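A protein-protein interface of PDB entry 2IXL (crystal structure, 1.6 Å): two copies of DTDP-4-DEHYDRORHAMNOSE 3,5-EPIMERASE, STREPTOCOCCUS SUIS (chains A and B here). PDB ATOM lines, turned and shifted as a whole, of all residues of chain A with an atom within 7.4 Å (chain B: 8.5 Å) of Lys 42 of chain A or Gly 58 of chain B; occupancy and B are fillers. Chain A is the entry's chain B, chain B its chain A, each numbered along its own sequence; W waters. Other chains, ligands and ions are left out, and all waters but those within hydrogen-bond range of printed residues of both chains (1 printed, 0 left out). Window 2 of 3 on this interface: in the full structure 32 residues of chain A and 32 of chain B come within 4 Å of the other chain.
The backbone carbonyl oxygen (O) of Gly 58 of chain B lies within hydrogen-bond range of the side-chain amino group (NZ) of Lys 42 of chain A (2.9 Å).
The backbone carbonyl oxygen (O) of Leu 60 of chain B is in hydrogen-bond range of the backbone NH (N) of Lys 42 of chain A.
The backbone NH (N) of Asn 62 of chain B sits at hydrogen-bond distance from the backbone carbonyl oxygen (O) of Phe 40 of chain A (2.8 Å).
The backbone NH of Leu 60 of chain B is in hydrogen-bond range of the side-chain hydroxyl of Tyr 145 of chain B (3.2 Å).
N of Val 142 of chain B lies within hydrogen-bond range of O of Gln 61 of chain B (2.9 Å).
OE1 of Gln 41 of chain A is in hydrogen-bond range of N of Glu 43 of chain A (2.9 Å).
The backbone NH (N) of Lys 44 of chain A lies within hydrogen-bond range of the side-chain amide oxygen (OE1) of Gln 41 of chain A, 2.9 Å away.
The backbone NH of Gln 41 of chain A is in hydrogen-bond range of the side-chain sulfur of Met 45 of chain A (3.5 Å).
Phe 40 of chain A touches Leu 60 of chain B.
Phe 40 of chain A touches Gln 61 of chain B (O to CA, 3.3 Å).
CG of Gln 41 of chain A touches NE2 of Gln 61 of chain B, 3.4 Å away.
NE2 of Gln 41 of chain A touches CD2 of Tyr 145 of chain B, 3.5 Å away.
CB of Lys 42 of chain A touches OH of Tyr 145 of chain B (3.4 Å).
Glu 43 of chain A touches Tyr 145 of chain B.
Lys 42 of chain A touches just these residues of chain B: Gly 58, Leu 60 and Tyr 145.
Gly 58 of chain B touches just one residue of chain A: Lys 42 (2.9 Å).
Of the printed residues of chain A, Leu 60 of chain B touches Phe 40 (3.8 Å) and Lys 42 (3.1 Å).
Printed residues of chain B within 4 Å of Phe 40 of chain A: Leu 60, Gln 61 and Asn 62.
Of the printed residues of chain B, Glu 43 of chain A touches Tyr 145.
Of the printed residues of chain A, Asn 62 of chain B touches Phe 40.
Of the printed residues of chain A, Gln 61 of chain B touches Phe 40 and Gln 41.
Pro 47 of chain A touches none of the printed residues of chain B.
Glu 52 of chain A touches none of the printed residues of chain B.
The nearest residue of chain B that does not touch Lys 42 of chain A is Lys 59 of chain B (4.8 Å).
The nearest residue of chain A that does not touch Gly 58 of chain B is Phe 55 of chain A (6.3 Å).
The nearest printed residue of chain A that does not touch Leu 60 of chain B is Gln 41 of chain A (4.1 Å).
Of the 15 printed residues of chain B, 5 touch a printed residue of chain A.
Along chain B the printed residues that touch a printed residue of chain A span positions 58 to 145.
Hydrophobic or aromatic side chains of chain A that line the printed part of chain B: Phe 40.
Among the printed residues, no Asp or Glu carboxylate lies within 4 Å of a Lys or Arg side-chain nitrogen of the other chain.
Positions printed for both chains: 52 and 55.
Water W1 bridges O of Gly 58 of chain B (3.0 Å) and NZ of Lys 42 of chain A (3.1 Å).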
ATOM      1  N   PHE A  40       0.457   4.182  -2.872  1.00  0.00           N
ATOM      2  CA  PHE A  40       0.224   5.237  -3.865  1.00  0.00           C
ATOM      3  C   PHE A  40       1.108   4.927  -5.072  1.00  0.00           C
ATOM      4  O   PHE A  40       2.276   4.581  -4.906  1.00  0.00           O
ATOM      5  CB  PHE A  40       0.581   6.632  -3.336  1.00  0.00           C
ATOM      6  CG  PHE A  40       0.461   7.707  -4.378  1.00  0.00           C
ATOM      7  CD1 PHE A  40      -0.790   8.206  -4.730  1.00  0.00           C
ATOM      8  CD2 PHE A  40       1.594   8.183  -5.048  1.00  0.00           C
ATOM      9  CE1 PHE A  40      -0.915   9.184  -5.719  1.00  0.00           C
ATOM     10  CE2 PHE A  40       1.481   9.171  -6.045  1.00  0.00           C
ATOM     11  CZ  PHE A  40       0.214   9.664  -6.382  1.00  0.00           C
ATOM     12  N   GLN A  41       0.549   5.039  -6.270  1.00  0.00           N
ATOM     13  CA  GLN A  41       1.306   4.790  -7.507  1.00  0.00           C
ATOM     14  C   GLN A  41       0.812   5.774  -8.575  1.00  0.00           C
ATOM     15  O   GLN A  41      -0.319   5.674  -9.052  1.00  0.00           O
ATOM     16  CB  GLN A  41       1.176   3.313  -7.919  1.00  0.00           C
ATOM     17  CG  GLN A  41       2.389   2.736  -8.691  1.00  0.00           C
ATOM     18  CD  GLN A  41       2.359   2.997 -10.189  1.00  0.00           C
ATOM     19  OE1 GLN A  41       1.828   4.016 -10.659  1.00  0.00           O
ATOM     20  NE2 GLN A  41       2.944   2.073 -10.953  1.00  0.00           N
ATOM     21  N   LYS A  42       1.655   6.763  -8.891  1.00  0.00           N
ATOM     22  CA  LYS A  42       1.213   7.941  -9.664  1.00  0.00           C
ATOM     23  C   LYS A  42       0.693   7.565 -11.050  1.00  0.00           C
ATOM     24  O   LYS A  42      -0.364   8.052 -11.476  1.00  0.00           O
ATOM     25  CB  LYS A  42       2.340   8.982  -9.761  1.00  0.00           C
ATOM     26  CG  LYS A  42       1.959  10.333 -10.398  1.00  0.00           C
ATOM     27  CD  LYS A  42       3.171  11.288 -10.414  1.00  0.00           C
ATOM     28  CE  LYS A  42       2.820  12.621 -11.079  1.00  0.00           C
ATOM     29  NZ  LYS A  42       4.041  13.515 -11.176  1.00  0.00           N
ATOM     30  N   GLU A  43       1.442   6.726 -11.758  1.00  0.00           N
ATOM     31  CA  GLU A  43       1.071   6.337 -13.123  1.00  0.00           C
ATOM     32  C   GLU A  43      -0.265   5.594 -13.203  1.00  0.00           C
ATOM     33  O   GLU A  43      -1.038   5.788 -14.152  1.00  0.00           O
ATOM     34  CB  GLU A  43       2.212   5.513 -13.734  1.00  0.00           C
ATOM     35  CG  GLU A  43       2.113   5.203 -15.205  1.00  0.00           C
ATOM     36  CD  GLU A  43       3.451   4.736 -15.757  1.00  0.00           C
ATOM     37  OE1 GLU A  43       3.758   3.544 -15.614  1.00  0.00           O
ATOM     38  OE2 GLU A  43       4.210   5.560 -16.312  1.00  0.00           O
ATOM     39  N   LYS A  44      -0.539   4.761 -12.195  1.00  0.00           N
ATOM     40  CA  LYS A  44      -1.788   3.985 -12.130  1.00  0.00           C
ATOM     41  C   LYS A  44      -2.985   4.773 -11.598  1.00  0.00           C
ATOM     42  O   LYS A  44      -4.135   4.431 -11.920  1.00  0.00           O
ATOM     43  CB  LYS A  44      -1.604   2.716 -11.282  1.00  0.00           C
ATOM     44  CG  LYS A  44      -0.591   1.720 -11.855  1.00  0.00           C
ATOM     45  CD  LYS A  44      -0.418   0.496 -10.933  1.00  0.00           C
ATOM     46  CE  LYS A  44       0.530  -0.572 -11.520  1.00  0.00           C
ATOM     47  NZ  LYS A  44       0.849  -1.683 -10.531  1.00  0.00           N
ATOM     48  N   MET A  45      -2.724   5.786 -10.760  1.00  0.00           N
ATOM     49  CA  MET A  45      -3.813   6.518 -10.088  1.00  0.00           C
ATOM     50  C   MET A  45      -4.328   7.767 -10.814  1.00  0.00           C
ATOM     51  O   MET A  45      -5.517   8.110 -10.696  1.00  0.00           O
ATOM     52  CB  MET A  45      -3.450   6.784  -8.616  1.00  0.00           C
ATOM     53  CG  MET A  45      -3.252   5.454  -7.874  1.00  0.00           C
ATOM     54  SD  MET A  45      -2.894   5.490  -6.112  1.00  0.00           S
ATOM     55  CE  MET A  45      -2.651   3.745  -5.787  1.00  0.00           C
ATOM     56  N   LEU A  46      -3.457   8.436 -11.567  1.00  0.00           N
ATOM     57  CA  LEU A  46      -3.900   9.558 -12.420  1.00  0.00           C
ATOM     58  C   LEU A  46      -5.075   9.196 -13.356  1.00  0.00           C
ATOM     59  O   LEU A  46      -6.055   9.959 -13.418  1.00  0.00           O
ATOM     60  CB  LEU A  46      -2.730  10.210 -13.196  1.00  0.00           C
ATOM     61  CG  LEU A  46      -1.655  10.987 -12.415  1.00  0.00           C
ATOM     62  CD1 LEU A  46      -0.710  11.746 -13.340  1.00  0.00           C
ATOM     63  CD2 LEU A  46      -2.261  11.936 -11.394  1.00  0.00           C
ATOM     64  N   PRO A  47      -5.003   8.054 -14.085  1.00  0.00           N
ATOM     65  CA  PRO A  47      -6.138   7.678 -14.963  1.00  0.00           C
ATOM     66  C   PRO A  47      -7.467   7.441 -14.232  1.00  0.00           C
ATOM     67  O   PRO A  47      -8.544   7.512 -14.865  1.00  0.00           O
ATOM     68  CB  PRO A  47      -5.649   6.389 -15.643  1.00  0.00           C
ATOM     69  CG  PRO A  47      -4.152   6.469 -15.574  1.00  0.00           C
ATOM     70  CD  PRO A  47      -3.892   7.094 -14.229  1.00  0.00           C
ATOM     71  N   LEU A  48      -7.398   7.164 -12.931  1.00  0.00           N
ATOM     72  CA  LEU A  48      -8.589   6.885 -12.114  1.00  0.00           C
ATOM     73  C   LEU A  48      -9.222   8.134 -11.479  1.00  0.00           C
ATOM     74  O   LEU A  48     -10.245   8.027 -10.785  1.00  0.00           O
ATOM     75  CB  LEU A  48      -8.257   5.863 -11.021  1.00  0.00           C
ATOM     76  CG  LEU A  48      -7.825   4.463 -11.468  1.00  0.00           C
ATOM     77  CD1 LEU A  48      -7.413   3.668 -10.251  1.00  0.00           C
ATOM     78  CD2 LEU A  48      -8.921   3.722 -12.277  1.00  0.00           C
ATOM     79  N   PHE A  50      -7.200  10.643  -9.570  1.00  0.00           N
ATOM     80  CA  PHE A  50      -6.290  11.381  -8.673  1.00  0.00           C
ATOM     81  C   PHE A  50      -5.823  12.650  -9.403  1.00  0.00           C
ATOM     82  O   PHE A  50      -5.251  12.554 -10.498  1.00  0.00           O
ATOM     83  CB  PHE A  50      -5.085  10.518  -8.234  1.00  0.00           C
ATOM     84  CG  PHE A  50      -4.307  11.099  -7.071  1.00  0.00           C
ATOM     85  CD1 PHE A  50      -4.500  10.630  -5.773  1.00  0.00           C
ATOM     86  CD2 PHE A  50      -3.386  12.127  -7.277  1.00  0.00           C
ATOM     87  CE1 PHE A  50      -3.777  11.169  -4.698  1.00  0.00           C
ATOM     88  CE2 PHE A  50      -2.665  12.685  -6.213  1.00  0.00           C
ATOM     89  CZ  PHE A  50      -2.860  12.200  -4.915  1.00  0.00           C
ATOM     90  N   PRO A  51      -6.087  13.842  -8.831  1.00  0.00           N
ATOM     91  CA  PRO A  51      -5.843  15.081  -9.594  1.00  0.00           C
ATOM     92  C   PRO A  51      -4.370  15.416  -9.851  1.00  0.00           C
ATOM     93  O   PRO A  51      -3.568  15.492  -8.909  1.00  0.00           O
ATOM     94  CB  PRO A  51      -6.504  16.169  -8.727  1.00  0.00           C
ATOM     95  CG  PRO A  51      -6.474  15.649  -7.396  1.00  0.00           C
ATOM     96  CD  PRO A  51      -6.650  14.136  -7.499  1.00  0.00           C
ATOM     97  N   GLU A  52      -4.022  15.622 -11.128  1.00  0.00           N
ATOM     98  CA  GLU A  52      -2.686  16.090 -11.519  1.00  0.00           C
ATOM     99  C   GLU A  52      -2.284  17.363 -10.773  1.00  0.00           C
ATOM    100  O   GLU A  52      -1.098  17.565 -10.468  1.00  0.00           O
ATOM    101  CB  GLU A  52      -2.627  16.385 -13.027  1.00  0.00           C
ATOM    102  CG  GLU A  52      -2.537  15.176 -13.936  1.00  0.00           C
ATOM    103  CD  GLU A  52      -1.936  15.526 -15.295  1.00  0.00           C
ATOM    104  OE1 GLU A  52      -2.614  16.183 -16.121  1.00  0.00           O
ATOM    105  OE2 GLU A  52      -0.769  15.148 -15.532  1.00  0.00           O
ATOM    106  N   PHE A  55       0.307  17.885  -7.844  1.00  0.00           N
ATOM    107  CA  PHE A  55       1.749  18.023  -8.069  1.00  0.00           C
ATOM    108  C   PHE A  55       2.175  19.389  -8.631  1.00  0.00           C
ATOM    109  O   PHE A  55       3.357  19.586  -8.961  1.00  0.00           O
ATOM    110  CB  PHE A  55       2.204  16.901  -9.013  1.00  0.00           C
ATOM    111  CG  PHE A  55       1.920  15.525  -8.477  1.00  0.00           C
ATOM    112  CD1 PHE A  55       0.787  14.824  -8.887  1.00  0.00           C
ATOM    113  CD2 PHE A  55       2.754  14.962  -7.529  1.00  0.00           C
ATOM    114  CE1 PHE A  55       0.514  13.547  -8.364  1.00  0.00           C
ATOM    115  CE2 PHE A  55       2.496  13.689  -7.003  1.00  0.00           C
ATOM    116  CZ  PHE A  55       1.377  12.988  -7.424  1.00  0.00           C
ATOM    117  N   GLU B  52      18.370  16.307  -4.819  1.00  0.00           N
ATOM    118  CA  GLU B  52      17.415  16.868  -5.781  1.00  0.00           C
ATOM    119  C   GLU B  52      17.189  15.919  -6.975  1.00  0.00           C
ATOM    120  O   GLU B  52      16.096  15.898  -7.557  1.00  0.00           O
ATOM    121  CB  GLU B  52      17.909  18.229  -6.293  1.00  0.00           C
ATOM    122  CG  GLU B  52      17.702  19.414  -5.327  1.00  0.00           C
ATOM    123  CD  GLU B  52      18.824  19.585  -4.303  1.00  0.00           C
ATOM    124  OE1 GLU B  52      19.730  18.723  -4.217  1.00  0.00           O
ATOM    125  OE2 GLU B  52      18.807  20.597  -3.570  1.00  0.00           O
ATOM    126  N   SER B  53      18.216  15.148  -7.335  1.00  0.00           N
ATOM    127  CA  SER B  53      18.123  14.186  -8.447  1.00  0.00           C
ATOM    128  C   SER B  53      17.034  13.106  -8.264  1.00  0.00           C
ATOM    129  O   SER B  53      16.607  12.490  -9.243  1.00  0.00           O
ATOM    130  CB  SER B  53      19.478  13.519  -8.720  1.00  0.00           C
ATOM    131  OG  SER B  53      19.887  12.727  -7.606  1.00  0.00           O
ATOM    132  N   PHE B  54      16.577  12.886  -7.030  1.00  0.00           N
ATOM    133  CA  PHE B  54      15.443  11.966  -6.788  1.00  0.00           C
ATOM    134  C   PHE B  54      14.213  12.366  -7.632  1.00  0.00           C
ATOM    135  O   PHE B  54      13.417  11.505  -8.049  1.00  0.00           O
ATOM    136  CB  PHE B  54      15.084  11.949  -5.292  1.00  0.00           C
ATOM    137  CG  PHE B  54      13.971  10.980  -4.923  1.00  0.00           C
ATOM    138  CD1 PHE B  54      14.246   9.635  -4.681  1.00  0.00           C
ATOM    139  CD2 PHE B  54      12.649  11.430  -4.771  1.00  0.00           C
ATOM    140  CE1 PHE B  54      13.227   8.752  -4.307  1.00  0.00           C
ATOM    141  CE2 PHE B  54      11.614  10.548  -4.410  1.00  0.00           C
ATOM    142  CZ  PHE B  54      11.904   9.216  -4.176  1.00  0.00           C
ATOM    143  N   PHE B  55      14.091  13.670  -7.911  1.00  0.00           N
ATOM    144  CA  PHE B  55      12.887  14.231  -8.546  1.00  0.00           C
ATOM    145  C   PHE B  55      13.005  14.407 -10.064  1.00  0.00           C
ATOM    146  O   PHE B  55      12.122  15.002 -10.695  1.00  0.00           O
ATOM    147  CB  PHE B  55      12.508  15.561  -7.860  1.00  0.00           C
ATOM    148  CG  PHE B  55      12.210  15.403  -6.391  1.00  0.00           C
ATOM    149  CD1 PHE B  55      13.210  15.589  -5.437  1.00  0.00           C
ATOM    150  CD2 PHE B  55      10.951  14.986  -5.972  1.00  0.00           C
ATOM    151  CE1 PHE B  55      12.948  15.411  -4.089  1.00  0.00           C
ATOM    152  CE2 PHE B  55      10.671  14.815  -4.610  1.00  0.00           C
ATOM    153  CZ  PHE B  55      11.679  15.023  -3.673  1.00  0.00           C
ATOM    154  N   ALA B  56      14.078  13.868 -10.649  1.00  0.00           N
ATOM    155  CA  ALA B  56      14.407  14.104 -12.071  1.00  0.00           C
ATOM    156  C   ALA B  56      13.295  13.774 -13.082  1.00  0.00           C
ATOM    157  O   ALA B  56      13.100  14.520 -14.037  1.00  0.00           O
ATOM    158  CB  ALA B  56      15.698  13.380 -12.454  1.00  0.00           C
ATOM    159  N   GLU B  57      12.589  12.659 -12.888  1.00  0.00           N
ATOM    160  CA  GLU B  57      11.572  12.219 -13.879  1.00  0.00           C
ATOM    161  C   GLU B  57      10.121  12.515 -13.465  1.00  0.00           C
ATOM    162  O   GLU B  57       9.175  12.225 -14.215  1.00  0.00           O
ATOM    163  CB  GLU B  57      11.722  10.726 -14.192  1.00  0.00           C
ATOM    164  CG  GLU B  57      13.027  10.362 -14.882  1.00  0.00           C
ATOM    165  CD  GLU B  57      13.039   8.933 -15.404  1.00  0.00           C
ATOM    166  OE1 GLU B  57      12.764   7.998 -14.625  1.00  0.00           O
ATOM    167  OE2 GLU B  57      13.336   8.745 -16.602  1.00  0.00           O
ATOM    168  N   GLY B  58       9.948  13.098 -12.285  1.00  0.00           N
ATOM    169  CA  GLY B  58       8.609  13.427 -11.785  1.00  0.00           C
ATOM    170  C   GLY B  58       7.776  12.186 -11.509  1.00  0.00           C
ATOM    171  O   GLY B  58       6.549  12.208 -11.666  1.00  0.00           O
ATOM    172  N   LYS B  59       8.444  11.116 -11.090  1.00  0.00           N
ATOM    173  CA  LYS B  59       7.778   9.839 -10.797  1.00  0.00           C
ATOM    174  C   LYS B  59       7.698   9.604  -9.279  1.00  0.00           C
ATOM    175  O   LYS B  59       8.614   9.986  -8.533  1.00  0.00           O
ATOM    176  CB  LYS B  59       8.531   8.679 -11.471  1.00  0.00           C
ATOM    177  CG  LYS B  59       8.434   8.658 -13.002  1.00  0.00           C
ATOM    178  CD  LYS B  59       9.244   7.516 -13.586  1.00  0.00           C
ATOM    179  CE  LYS B  59       9.130   7.483 -15.098  1.00  0.00           C
ATOM    180  NZ  LYS B  59      10.024   6.449 -15.703  1.00  0.00           N
ATOM    181  N   LEU B  60       6.605   8.995  -8.815  1.00  0.00           N
ATOM    182  CA  LEU B  60       6.419   8.762  -7.371  1.00  0.00           C
ATOM    183  C   LEU B  60       5.563   7.532  -7.085  1.00  0.00           C
ATOM    184  O   LEU B  60       4.477   7.379  -7.641  1.00  0.00           O
ATOM    185  CB  LEU B  60       5.794   9.990  -6.680  1.00  0.00           C
ATOM    186  CG  LEU B  60       5.712   9.965  -5.151  1.00  0.00           C
ATOM    187  CD1 LEU B  60       7.115   9.962  -4.507  1.00  0.00           C
ATOM    188  CD2 LEU B  60       4.853  11.116  -4.631  1.00  0.00           C
ATOM    189  N   GLN B  61       6.067   6.676  -6.203  1.00  0.00           N
ATOM    190  CA  GLN B  61       5.324   5.508  -5.687  1.00  0.00           C
ATOM    191  C   GLN B  61       5.662   5.325  -4.204  1.00  0.00           C
ATOM    192  O   GLN B  61       6.813   5.506  -3.789  1.00  0.00           O
ATOM    193  CB  GLN B  61       5.687   4.245  -6.485  1.00  0.00           C
ATOM    194  CG  GLN B  61       5.059   2.925  -5.998  1.00  0.00           C
ATOM    195  CD  GLN B  61       5.362   1.729  -6.884  1.00  0.00           C
ATOM    196  OE1 GLN B  61       5.266   0.578  -6.438  1.00  0.00           O
ATOM    197  NE2 GLN B  61       5.698   1.975  -8.132  1.00  0.00           N
ATOM    198  N   ASN B  62       4.650   4.989  -3.412  1.00  0.00           N
ATOM    199  CA  ASN B  62       4.819   4.705  -1.981  1.00  0.00           C
ATOM    200  C   ASN B  62       4.380   3.277  -1.710  1.00  0.00           C
ATOM    201  O   ASN B  62       3.207   2.955  -1.906  1.00  0.00           O
ATOM    202  CB  ASN B  62       3.985   5.698  -1.144  1.00  0.00           C
ATOM    203  CG  ASN B  62       3.948   5.356   0.363  1.00  0.00           C
ATOM    204  OD1 ASN B  62       4.915   4.832   0.949  1.00  0.00           O
ATOM    205  ND2 ASN B  62       2.816   5.651   0.988  1.00  0.00           N
ATOM    206  N   VAL B 142       9.696   5.687  -3.638  1.00  0.00           N
ATOM    207  CA  VAL B 142      10.571   5.328  -4.771  1.00  0.00           C
ATOM    208  C   VAL B 142      10.242   6.166  -6.012  1.00  0.00           C
ATOM    209  O   VAL B 142       9.158   6.750  -6.090  1.00  0.00           O
ATOM    210  CB  VAL B 142      10.495   3.817  -5.106  1.00  0.00           C
ATOM    211  CG1 VAL B 142      10.782   2.978  -3.872  1.00  0.00           C
ATOM    212  CG2 VAL B 142       9.157   3.442  -5.747  1.00  0.00           C
ATOM    213  N   ASN B 143      11.171   6.225  -6.979  1.00  0.00           N
ATOM    214  CA  ASN B 143      11.025   7.135  -8.146  1.00  0.00           C
ATOM    215  C   ASN B 143      11.046   6.483  -9.552  1.00  0.00           C
ATOM    216  O   ASN B 143      11.378   7.130 -10.560  1.00  0.00           O
ATOM    217  CB  ASN B 143      12.062   8.275  -8.074  1.00  0.00           C
ATOM    218  CG  ASN B 143      13.484   7.764  -8.147  1.00  0.00           C
ATOM    219  OD1 ASN B 143      13.712   6.544  -8.121  1.00  0.00           O
ATOM    220  ND2 ASN B 143      14.456   8.679  -8.260  1.00  0.00           N
ATOM    221  N   ASP B 144      10.680   5.203  -9.619  1.00  0.00           N
ATOM    222  CA  ASP B 144      10.291   4.575 -10.886  1.00  0.00           C
ATOM    223  C   ASP B 144       9.334   3.422 -10.560  1.00  0.00           C
ATOM    224  O   ASP B 144       9.153   3.083  -9.379  1.00  0.00           O
ATOM    225  CB  ASP B 144      11.500   4.096 -11.715  1.00  0.00           C
ATOM    226  CG  ASP B 144      11.238   4.154 -13.238  1.00  0.00           C
ATOM    227  OD1 ASP B 144      10.057   4.196 -13.649  1.00  0.00           O
ATOM    228  OD2 ASP B 144      12.214   4.199 -14.038  1.00  0.00           O
ATOM    229  N   TYR B 145       8.735   2.850 -11.610  1.00  0.00           N
ATOM    230  CA  TYR B 145       7.602   1.916 -11.486  1.00  0.00           C
ATOM    231  C   TYR B 145       7.946   0.448 -11.817  1.00  0.00           C
ATOM    232  O   TYR B 145       8.341   0.111 -12.944  1.00  0.00           O
ATOM    233  CB  TYR B 145       6.410   2.400 -12.344  1.00  0.00           C
ATOM    234  CG  TYR B 145       6.041   3.870 -12.113  1.00  0.00           C
ATOM    235  CD1 TYR B 145       6.108   4.806 -13.151  1.00  0.00           C
ATOM    236  CD2 TYR B 145       5.665   4.325 -10.834  1.00  0.00           C
ATOM    237  CE1 TYR B 145       5.774   6.169 -12.918  1.00  0.00           C
ATOM    238  CE2 TYR B 145       5.358   5.666 -10.591  1.00  0.00           C
ATOM    239  CZ  TYR B 145       5.403   6.583 -11.635  1.00  0.00           C
ATOM    240  OH  TYR B 145       5.077   7.912 -11.370  1.00  0.00           O
HETATM  241  O   HOH W   1       5.227  13.414 -14.091  1.00  0.00           O
